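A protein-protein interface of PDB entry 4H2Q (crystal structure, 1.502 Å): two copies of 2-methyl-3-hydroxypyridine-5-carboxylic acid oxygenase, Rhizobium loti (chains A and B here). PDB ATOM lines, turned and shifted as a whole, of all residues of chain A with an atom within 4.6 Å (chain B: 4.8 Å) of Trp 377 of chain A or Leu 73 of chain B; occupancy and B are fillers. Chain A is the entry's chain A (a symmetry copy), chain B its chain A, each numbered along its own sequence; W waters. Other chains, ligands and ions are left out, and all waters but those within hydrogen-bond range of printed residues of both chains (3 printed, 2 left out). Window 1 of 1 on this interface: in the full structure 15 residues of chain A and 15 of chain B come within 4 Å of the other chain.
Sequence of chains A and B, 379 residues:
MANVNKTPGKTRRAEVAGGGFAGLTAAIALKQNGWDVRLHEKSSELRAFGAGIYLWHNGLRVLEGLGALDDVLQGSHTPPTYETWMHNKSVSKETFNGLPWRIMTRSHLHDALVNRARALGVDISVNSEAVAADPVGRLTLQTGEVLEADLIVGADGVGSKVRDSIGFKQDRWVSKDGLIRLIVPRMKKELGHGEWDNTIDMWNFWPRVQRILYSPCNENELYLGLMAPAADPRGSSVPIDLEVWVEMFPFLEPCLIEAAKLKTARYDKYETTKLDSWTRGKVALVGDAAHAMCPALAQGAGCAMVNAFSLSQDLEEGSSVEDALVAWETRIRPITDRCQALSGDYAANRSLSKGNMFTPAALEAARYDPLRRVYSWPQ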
ATOM      1  N   HIS A  57     -32.917  -5.165   8.382  1.00  0.00           N
ATOM      2  CA  HIS A  57     -32.842  -4.795   9.789  1.00  0.00           C
ATOM      3  C   HIS A  57     -34.167  -4.275  10.352  1.00  0.00           C
ATOM      4  O   HIS A  57     -34.618  -4.752  11.393  1.00  0.00           O
ATOM      5  CB  HIS A  57     -31.710  -3.773   9.961  1.00  0.00           C
ATOM      6  CG  HIS A  57     -31.767  -2.976  11.225  1.00  0.00           C
ATOM      7  ND1 HIS A  57     -32.225  -1.678  11.258  1.00  0.00           N
ATOM      8  CD2 HIS A  57     -31.371  -3.268  12.489  1.00  0.00           C
ATOM      9  CE1 HIS A  57     -32.141  -1.212  12.494  1.00  0.00           C
ATOM     10  NE2 HIS A  57     -31.626  -2.157  13.262  1.00  0.00           N
ATOM     11  N   ASN A  97     -22.305  -2.612   4.990  1.00  0.00           N
ATOM     12  CA  ASN A  97     -21.620  -2.340   6.239  1.00  0.00           C
ATOM     13  C   ASN A  97     -22.259  -3.060   7.433  1.00  0.00           C
ATOM     14  O   ASN A  97     -22.480  -2.445   8.492  1.00  0.00           O
ATOM     15  CB  ASN A  97     -21.570  -0.822   6.453  1.00  0.00           C
ATOM     16  CG  ASN A  97     -20.849  -0.106   5.321  1.00  0.00           C
ATOM     17  OD1 ASN A  97     -19.615  -0.138   5.246  1.00  0.00           O
ATOM     18  ND2 ASN A  97     -21.607   0.533   4.428  1.00  0.00           N
ATOM     19  N   GLY A  98     -22.595  -4.330   7.242  1.00  0.00           N
ATOM     20  CA  GLY A  98     -23.100  -5.149   8.324  1.00  0.00           C
ATOM     21  C   GLY A  98     -24.579  -5.067   8.627  1.00  0.00           C
ATOM     22  O   GLY A  98     -25.065  -5.809   9.476  1.00  0.00           O
ATOM     23  N   LEU A  99     -25.296  -4.164   7.964  1.00  0.00           N
ATOM     24  CA  LEU A  99     -26.738  -4.043   8.140  1.00  0.00           C
ATOM     25  C   LEU A  99     -27.404  -5.410   7.957  1.00  0.00           C
ATOM     26  O   LEU A  99     -27.261  -6.023   6.906  1.00  0.00           O
ATOM     27  CB  LEU A  99     -27.291  -3.058   7.107  1.00  0.00           C
ATOM     28  CG  LEU A  99     -28.804  -2.851   7.023  1.00  0.00           C
ATOM     29  CD1 LEU A  99     -29.282  -1.946   8.141  1.00  0.00           C
ATOM     30  CD2 LEU A  99     -29.179  -2.259   5.680  1.00  0.00           C
ATOM     31  N   PRO A 100     -28.140  -5.890   8.980  1.00  0.00           N
ATOM     32  CA  PRO A 100     -28.739  -7.228   8.847  1.00  0.00           C
ATOM     33  C   PRO A 100     -29.782  -7.318   7.742  1.00  0.00           C
ATOM     34  O   PRO A 100     -30.519  -6.369   7.504  1.00  0.00           O
ATOM     35  CB  PRO A 100     -29.404  -7.449  10.207  1.00  0.00           C
ATOM     36  CG  PRO A 100     -28.570  -6.621  11.161  1.00  0.00           C
ATOM     37  CD  PRO A 100     -28.161  -5.403  10.371  1.00  0.00           C
ATOM     38  N   ARG A 367     -32.445   0.973   7.717  1.00  0.00           N
ATOM     39  CA  ARG A 367     -31.646   1.378   8.871  1.00  0.00           C
ATOM     40  C   ARG A 367     -32.490   1.733  10.081  1.00  0.00           C
ATOM     41  O   ARG A 367     -31.991   1.727  11.213  1.00  0.00           O
ATOM     42  CB  ARG A 367     -30.742   2.561   8.504  1.00  0.00           C
ATOM     43  CG  ARG A 367     -29.650   2.211   7.479  1.00  0.00           C
ATOM     44  CD  ARG A 367     -28.777   3.401   7.163  1.00  0.00           C
ATOM     45  NE  ARG A 367     -28.179   3.846   8.409  1.00  0.00           N
ATOM     46  CZ  ARG A 367     -28.388   5.035   8.955  1.00  0.00           C
ATOM     47  NH1 ARG A 367     -29.152   5.929   8.332  1.00  0.00           N
ATOM     48  NH2 ARG A 367     -27.827   5.325  10.121  1.00  0.00           N
ATOM     49  N   SER A 376     -29.979   2.934  12.853  1.00  0.00           N
ATOM     50  CA  SER A 376     -28.787   2.179  13.250  1.00  0.00           C
ATOM     51  C   SER A 376     -27.966   1.829  12.009  1.00  0.00           C
ATOM     52  O   SER A 376     -28.230   2.342  10.917  1.00  0.00           O
ATOM     53  CB  SER A 376     -29.199   0.921  14.034  1.00  0.00           C
ATOM     54  OG  SER A 376     -28.088   0.251  14.629  1.00  0.00           O
ATOM     55  N   TRP A 377     -26.960   0.975  12.175  1.00  0.00           N
ATOM     56  CA  TRP A 377     -26.139   0.483  11.058  1.00  0.00           C
ATOM     57  C   TRP A 377     -25.742   1.554  10.048  1.00  0.00           C
ATOM     58  O   TRP A 377     -26.137   1.512   8.875  1.00  0.00           O
ATOM     59  CB  TRP A 377     -26.821  -0.717  10.397  1.00  0.00           C
ATOM     60  CG  TRP A 377     -26.993  -1.798  11.393  1.00  0.00           C
ATOM     61  CD1 TRP A 377     -28.126  -2.099  12.103  1.00  0.00           C
ATOM     62  CD2 TRP A 377     -25.980  -2.698  11.846  1.00  0.00           C
ATOM     63  NE1 TRP A 377     -27.876  -3.146  12.957  1.00  0.00           N
ATOM     64  CE2 TRP A 377     -26.566  -3.528  12.826  1.00  0.00           C
ATOM     65  CE3 TRP A 377     -24.627  -2.883  11.523  1.00  0.00           C
ATOM     66  CZ2 TRP A 377     -25.849  -4.537  13.475  1.00  0.00           C
ATOM     67  CZ3 TRP A 377     -23.919  -3.883  12.166  1.00  0.00           C
ATOM     68  CH2 TRP A 377     -24.530  -4.696  13.132  1.00  0.00           C
ATOM     69  N   PRO A 378     -24.970   2.539  10.507  1.00  0.00           N
ATOM     70  CA  PRO A 378     -24.580   3.660   9.648  1.00  0.00           C
ATOM     71  C   PRO A 378     -23.735   3.209   8.465  1.00  0.00           C
ATOM     72  O   PRO A 378     -22.985   2.238   8.551  1.00  0.00           O
ATOM     73  CB  PRO A 378     -23.770   4.553  10.594  1.00  0.00           C
ATOM     74  CG  PRO A 378     -23.240   3.605  11.635  1.00  0.00           C
ATOM     75  CD  PRO A 378     -24.370   2.642  11.852  1.00  0.00           C
ATOM     76  N   GLN A 379     -23.863   3.929   7.358  1.00  0.00           N
ATOM     77  CA  GLN A 379     -23.202   3.540   6.128  1.00  0.00           C
ATOM     78  C   GLN A 379     -21.967   4.391   5.855  1.00  0.00           C
ATOM     79  O   GLN A 379     -21.713   5.376   6.552  1.00  0.00           O
ATOM     80  CB  GLN A 379     -24.205   3.639   4.981  1.00  0.00           C
ATOM     81  CG  GLN A 379     -25.404   2.737   5.193  1.00  0.00           C
ATOM     82  CD  GLN A 379     -25.015   1.271   5.153  1.00  0.00           C
ATOM     83  OE1 GLN A 379     -24.454   0.804   4.168  1.00  0.00           O
ATOM     84  NE2 GLN A 379     -25.291   0.546   6.235  1.00  0.00           N
ATOM     85  OXT GLN A 379     -21.189   4.108   4.943  1.00  0.00           O
ATOM     86  N   LEU B  60     -22.177  -7.217  20.696  1.00  0.00           N
ATOM     87  CA  LEU B  60     -22.984  -6.128  20.159  1.00  0.00           C
ATOM     88  C   LEU B  60     -24.324  -6.033  20.891  1.00  0.00           C
ATOM     89  O   LEU B  60     -24.845  -4.928  21.106  1.00  0.00           O
ATOM     90  CB  LEU B  60     -23.180  -6.290  18.647  1.00  0.00           C
ATOM     91  CG  LEU B  60     -21.884  -6.223  17.840  1.00  0.00           C
ATOM     92  CD1 LEU B  60     -22.134  -6.669  16.409  1.00  0.00           C
ATOM     93  CD2 LEU B  60     -21.322  -4.825  17.857  1.00  0.00           C
ATOM     94  N   LEU B  69     -24.414   1.000  21.853  1.00  0.00           N
ATOM     95  CA  LEU B  69     -24.257   0.408  20.529  1.00  0.00           C
ATOM     96  C   LEU B  69     -24.073   1.454  19.423  1.00  0.00           C
ATOM     97  O   LEU B  69     -23.216   1.286  18.552  1.00  0.00           O
ATOM     98  CB  LEU B  69     -25.434  -0.508  20.186  1.00  0.00           C
ATOM     99  CG  LEU B  69     -25.374  -1.145  18.791  1.00  0.00           C
ATOM    100  CD1 LEU B  69     -24.219  -2.134  18.702  1.00  0.00           C
ATOM    101  CD2 LEU B  69     -26.704  -1.801  18.433  1.00  0.00           C
ATOM    102  N   ASP B  70     -24.886   2.511  19.451  1.00  0.00           N
ATOM    103  CA  ASP B  70     -24.834   3.551  18.423  1.00  0.00           C
ATOM    104  C   ASP B  70     -23.439   4.147  18.253  1.00  0.00           C
ATOM    105  O   ASP B  70     -22.928   4.263  17.130  1.00  0.00           O
ATOM    106  CB  ASP B  70     -25.832   4.673  18.736  1.00  0.00           C
ATOM    107  CG  ASP B  70     -27.274   4.183  18.789  1.00  0.00           C
ATOM    108  OD1 ASP B  70     -27.607   3.197  18.098  1.00  0.00           O
ATOM    109  OD2 ASP B  70     -28.080   4.796  19.524  1.00  0.00           O
ATOM    110  N   ASP B  71     -22.817   4.516  19.366  1.00  0.00           N
ATOM    111  CA  ASP B  71     -21.496   5.124  19.323  1.00  0.00           C
ATOM    112  C   ASP B  71     -20.451   4.145  18.811  1.00  0.00           C
ATOM    113  O   ASP B  71     -19.459   4.553  18.208  1.00  0.00           O
ATOM    114  CB  ASP B  71     -21.076   5.627  20.710  1.00  0.00           C
ATOM    115  CG  ASP B  71     -21.699   6.961  21.065  1.00  0.00           C
ATOM    116  OD1 ASP B  71     -22.288   7.609  20.175  1.00  0.00           O
ATOM    117  OD2 ASP B  71     -21.589   7.361  22.247  1.00  0.00           O
ATOM    118  N   VAL B  72     -20.660   2.857  19.070  1.00  0.00           N
ATOM    119  CA  VAL B  72     -19.729   1.851  18.590  1.00  0.00           C
ATOM    120  C   VAL B  72     -19.867   1.620  17.078  1.00  0.00           C
ATOM    121  O   VAL B  72     -18.873   1.639  16.362  1.00  0.00           O
ATOM    122  CB  VAL B  72     -19.850   0.535  19.386  1.00  0.00           C
ATOM    123  CG1 VAL B  72     -19.112  -0.584  18.691  1.00  0.00           C
ATOM    124  CG2 VAL B  72     -19.295   0.730  20.805  1.00  0.00           C
ATOM    125  N   LEU B  73     -21.094   1.423  16.593  1.00  0.00           N
ATOM    126  CA  LEU B  73     -21.292   1.140  15.172  1.00  0.00           C
ATOM    127  C   LEU B  73     -20.839   2.303  14.287  1.00  0.00           C
ATOM    128  O   LEU B  73     -20.265   2.098  13.222  1.00  0.00           O
ATOM    129  CB  LEU B  73     -22.752   0.779  14.884  1.00  0.00           C
ATOM    130  CG  LEU B  73     -23.268  -0.517  15.504  1.00  0.00           C
ATOM    131  CD1 LEU B  73     -24.704  -0.769  15.046  1.00  0.00           C
ATOM    132  CD2 LEU B  73     -22.373  -1.691  15.142  1.00  0.00           C
ATOM    133  N   GLN B  74     -21.086   3.527  14.732  1.00  0.00           N
ATOM    134  CA  GLN B  74     -20.535   4.685  14.047  1.00  0.00           C
ATOM    135  C   GLN B  74     -19.015   4.671  14.136  1.00  0.00           C
ATOM    136  O   GLN B  74     -18.458   4.687  15.233  1.00  0.00           O
ATOM    137  CB  GLN B  74     -21.090   5.966  14.672  1.00  0.00           C
ATOM    138  CG  GLN B  74     -20.584   7.234  14.008  1.00  0.00           C
ATOM    139  CD  GLN B  74     -21.095   7.390  12.584  1.00  0.00           C
ATOM    140  OE1 GLN B  74     -20.331   7.710  11.673  1.00  0.00           O
ATOM    141  NE2 GLN B  74     -22.390   7.169  12.389  1.00  0.00           N
ATOM    142  N   GLY B  75     -18.338   4.597  12.995  1.00  0.00           N
ATOM    143  CA  GLY B  75     -16.885   4.621  12.994  1.00  0.00           C
ATOM    144  C   GLY B  75     -16.195   3.281  13.192  1.00  0.00           C
ATOM    145  O   GLY B  75     -14.992   3.236  13.485  1.00  0.00           O
ATOM    146  N   SER B  76     -16.948   2.195  13.021  1.00  0.00           N
ATOM    147  CA  SER B  76     -16.376   0.850  13.007  1.00  0.00           C
ATOM    148  C   SER B  76     -16.853   0.128  11.747  1.00  0.00           C
ATOM    149  O   SER B  76     -17.632   0.684  10.978  1.00  0.00           O
ATOM    150  CB  SER B  76     -16.758   0.079  14.273  1.00  0.00           C
ATOM    151  OG  SER B  76     -18.164  -0.046  14.375  1.00  0.00           O
ATOM    152  N   THR B  78     -17.894  -3.587   9.450  1.00  0.00           N
ATOM    153  CA  THR B  78     -18.125  -5.021   9.256  1.00  0.00           C
ATOM    154  C   THR B  78     -17.571  -5.384   7.892  1.00  0.00           C
ATOM    155  O   THR B  78     -18.083  -4.928   6.874  1.00  0.00           O
ATOM    156  CB  THR B  78     -19.628  -5.435   9.292  1.00  0.00           C
ATOM    157  OG1 THR B  78     -20.223  -5.071  10.546  1.00  0.00           O
ATOM    158  CG2 THR B  78     -19.769  -6.941   9.109  1.00  0.00           C
ATOM    159  N   PRO B 100     -24.217 -11.036  13.182  1.00  0.00           N
ATOM    160  CA  PRO B 100     -23.541  -9.729  13.207  1.00  0.00           C
ATOM    161  C   PRO B 100     -22.144  -9.779  13.808  1.00  0.00           C
ATOM    162  O   PRO B 100     -21.896 -10.534  14.741  1.00  0.00           O
ATOM    163  CB  PRO B 100     -24.457  -8.879  14.091  1.00  0.00           C
ATOM    164  CG  PRO B 100     -25.826  -9.495  13.897  1.00  0.00           C
ATOM    165  CD  PRO B 100     -25.575 -10.975  13.750  1.00  0.00           C
ATOM    166  N   ARG B 102     -18.217  -7.140  14.031  1.00  0.00           N
ATOM    167  CA  ARG B 102     -17.717  -5.783  13.870  1.00  0.00           C
ATOM    168  C   ARG B 102     -16.254  -5.727  14.267  1.00  0.00           C
ATOM    169  O   ARG B 102     -15.833  -6.415  15.199  1.00  0.00           O
ATOM    170  CB  ARG B 102     -18.514  -4.831  14.769  1.00  0.00           C
ATOM    171  CG  ARG B 102     -18.508  -3.371  14.317  1.00  0.00           C
ATOM    172  CD  ARG B 102     -19.297  -3.216  13.031  1.00  0.00           C
ATOM    173  NE  ARG B 102     -19.608  -1.823  12.755  1.00  0.00           N
ATOM    174  CZ  ARG B 102     -20.414  -1.446  11.771  1.00  0.00           C
ATOM    175  NH1 ARG B 102     -20.951  -2.376  10.987  1.00  0.00           N
ATOM    176  NH2 ARG B 102     -20.692  -0.159  11.573  1.00  0.00           N
HETATM  177  O   HOH W   1     -20.506  -5.700   5.551  1.00  0.00           O
HETATM  178  O   HOH W   2     -22.777  -7.434  10.849  1.00  0.00           O
HETATM  179  O   HOH W   3     -23.154  -0.121   9.852  1.00  0.00           O
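Of the printed residues of chain B, Ser 376 of chain A touches Leu 73 (3.6 Å).
Trp 377 of chain A touches just these residues of chain B: Leu 73 (3.9 Å) and Arg 102 (3.5 Å).
Gln 379 of chain A touches none of the printed residues of chain B.
Leu 73 of chain B touches just these residues of chain A: Ser 376, Trp 377 and Pro 378.
Printed residues of chain A within 4 Å of Gln 74 of chain B: Pro 378 (3.5 Å).
The nearest residue of chain B that does not touch Trp 377 of chain A is Thr 78 of chain B (4.2 Å).
The nearest printed residue of chain A that does not touch Leu 73 of chain B is Asn 97 of chain A (6.7 Å).
The nearest printed residue of chain A that does not touch Gln 74 of chain B is Gln 379 of chain A (5.8 Å).
Water W3 lies within hydrogen-bond range of the backbone carbonyl oxygen (O) of Pro 378 of chain A (2.7 Å), the backbone carbonyl oxygen (O) of Asn 97 of chain A (2.8 Å) and the guanidinium group (NH2) of Arg 102 of chain B (3.0 Å).
Water W1 bridges O of Thr 78 of chain B (2.9 Å) and N of Gly 98 of chain A (3.0 Å).
Water W2 lies within hydrogen-bond range of the backbone carbonyl oxygen (O) of Gly 98 of chain A (3.1 Å) and the side-chain hydroxyl (OG1) of Thr 78 of chain B (3.5 Å).
Of the 10 printed residues of chain A, 5 touch a printed residue of chain B.
Printed residues of chain A that touch a printed residue of chain B: Asn 97, Gly 98, Ser 376, Trp 377 and Pro 378.
Hydrophobic or aromatic side chains of chain A within 4 Å of the printed part of chain B: Trp 377 and Pro 378.
Hydrophobic or aromatic side chains of chain B within 4 Å of the printed part of chain A: Leu 73.
Among the printed residues, 7 pairs touch across the chains.
Among the printed residues, no Asp or Glu carboxylate lies within 4 Å of a Lys or Arg side-chain nitrogen of the other chain.
Position printed for both chains: 100.
The backbone NH (N) of Ser 376 of chain A is in hydrogen-bond range of the backbone carbonyl oxygen (O) of Arg 367 of chain A (2.9 Å).
ND2 of Asn 97 of chain A lies within hydrogen-bond range of OE1 of Gln 379 of chain A, 2.9 Å away.
The side-chain amide nitrogen of Gln 379 of chain A lies within hydrogen-bond range of the backbone carbonyl oxygen of Trp 377 of chain A.
The backbone carbonyl oxygen of Trp 377 of chain A is in hydrogen-bond range of the guanidinium group of Arg 367 of chain A, at 3.1 Å.
The side-chain hydroxyl (OG) of Ser 76 of chain B is in hydrogen-bond range of the guanidinium group (NE) of Arg 102 of chain B.
OG1 of Thr 78 of chain B lies within hydrogen-bond range of NH1 of Arg 102 of chain B, 2.8 Å away.
The guanidinium group (NH1) of Arg 102 of chain B is in hydrogen-bond range of the backbone carbonyl oxygen (O) of Asn 97 of chain A, at 2.9 Å.
Gly 98 of chain A touches Thr 78 of chain B (CA to CB, 3.6 Å).
OG of Ser 376 of chain A touches CD1 of Leu 73 of chain B, at 3.6 Å.
CD1 of Leu 73 of chain B touches CD2 of Trp 377 of chain A (3.9 Å).
Trp 377 of chain A touches Arg 102 of chain B.
Leu 73 of chain B touches Pro 378 of chain A.
NE2 of Gln 74 of chain B touches CB of Pro 378 of chain A, 3.5 Å away.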
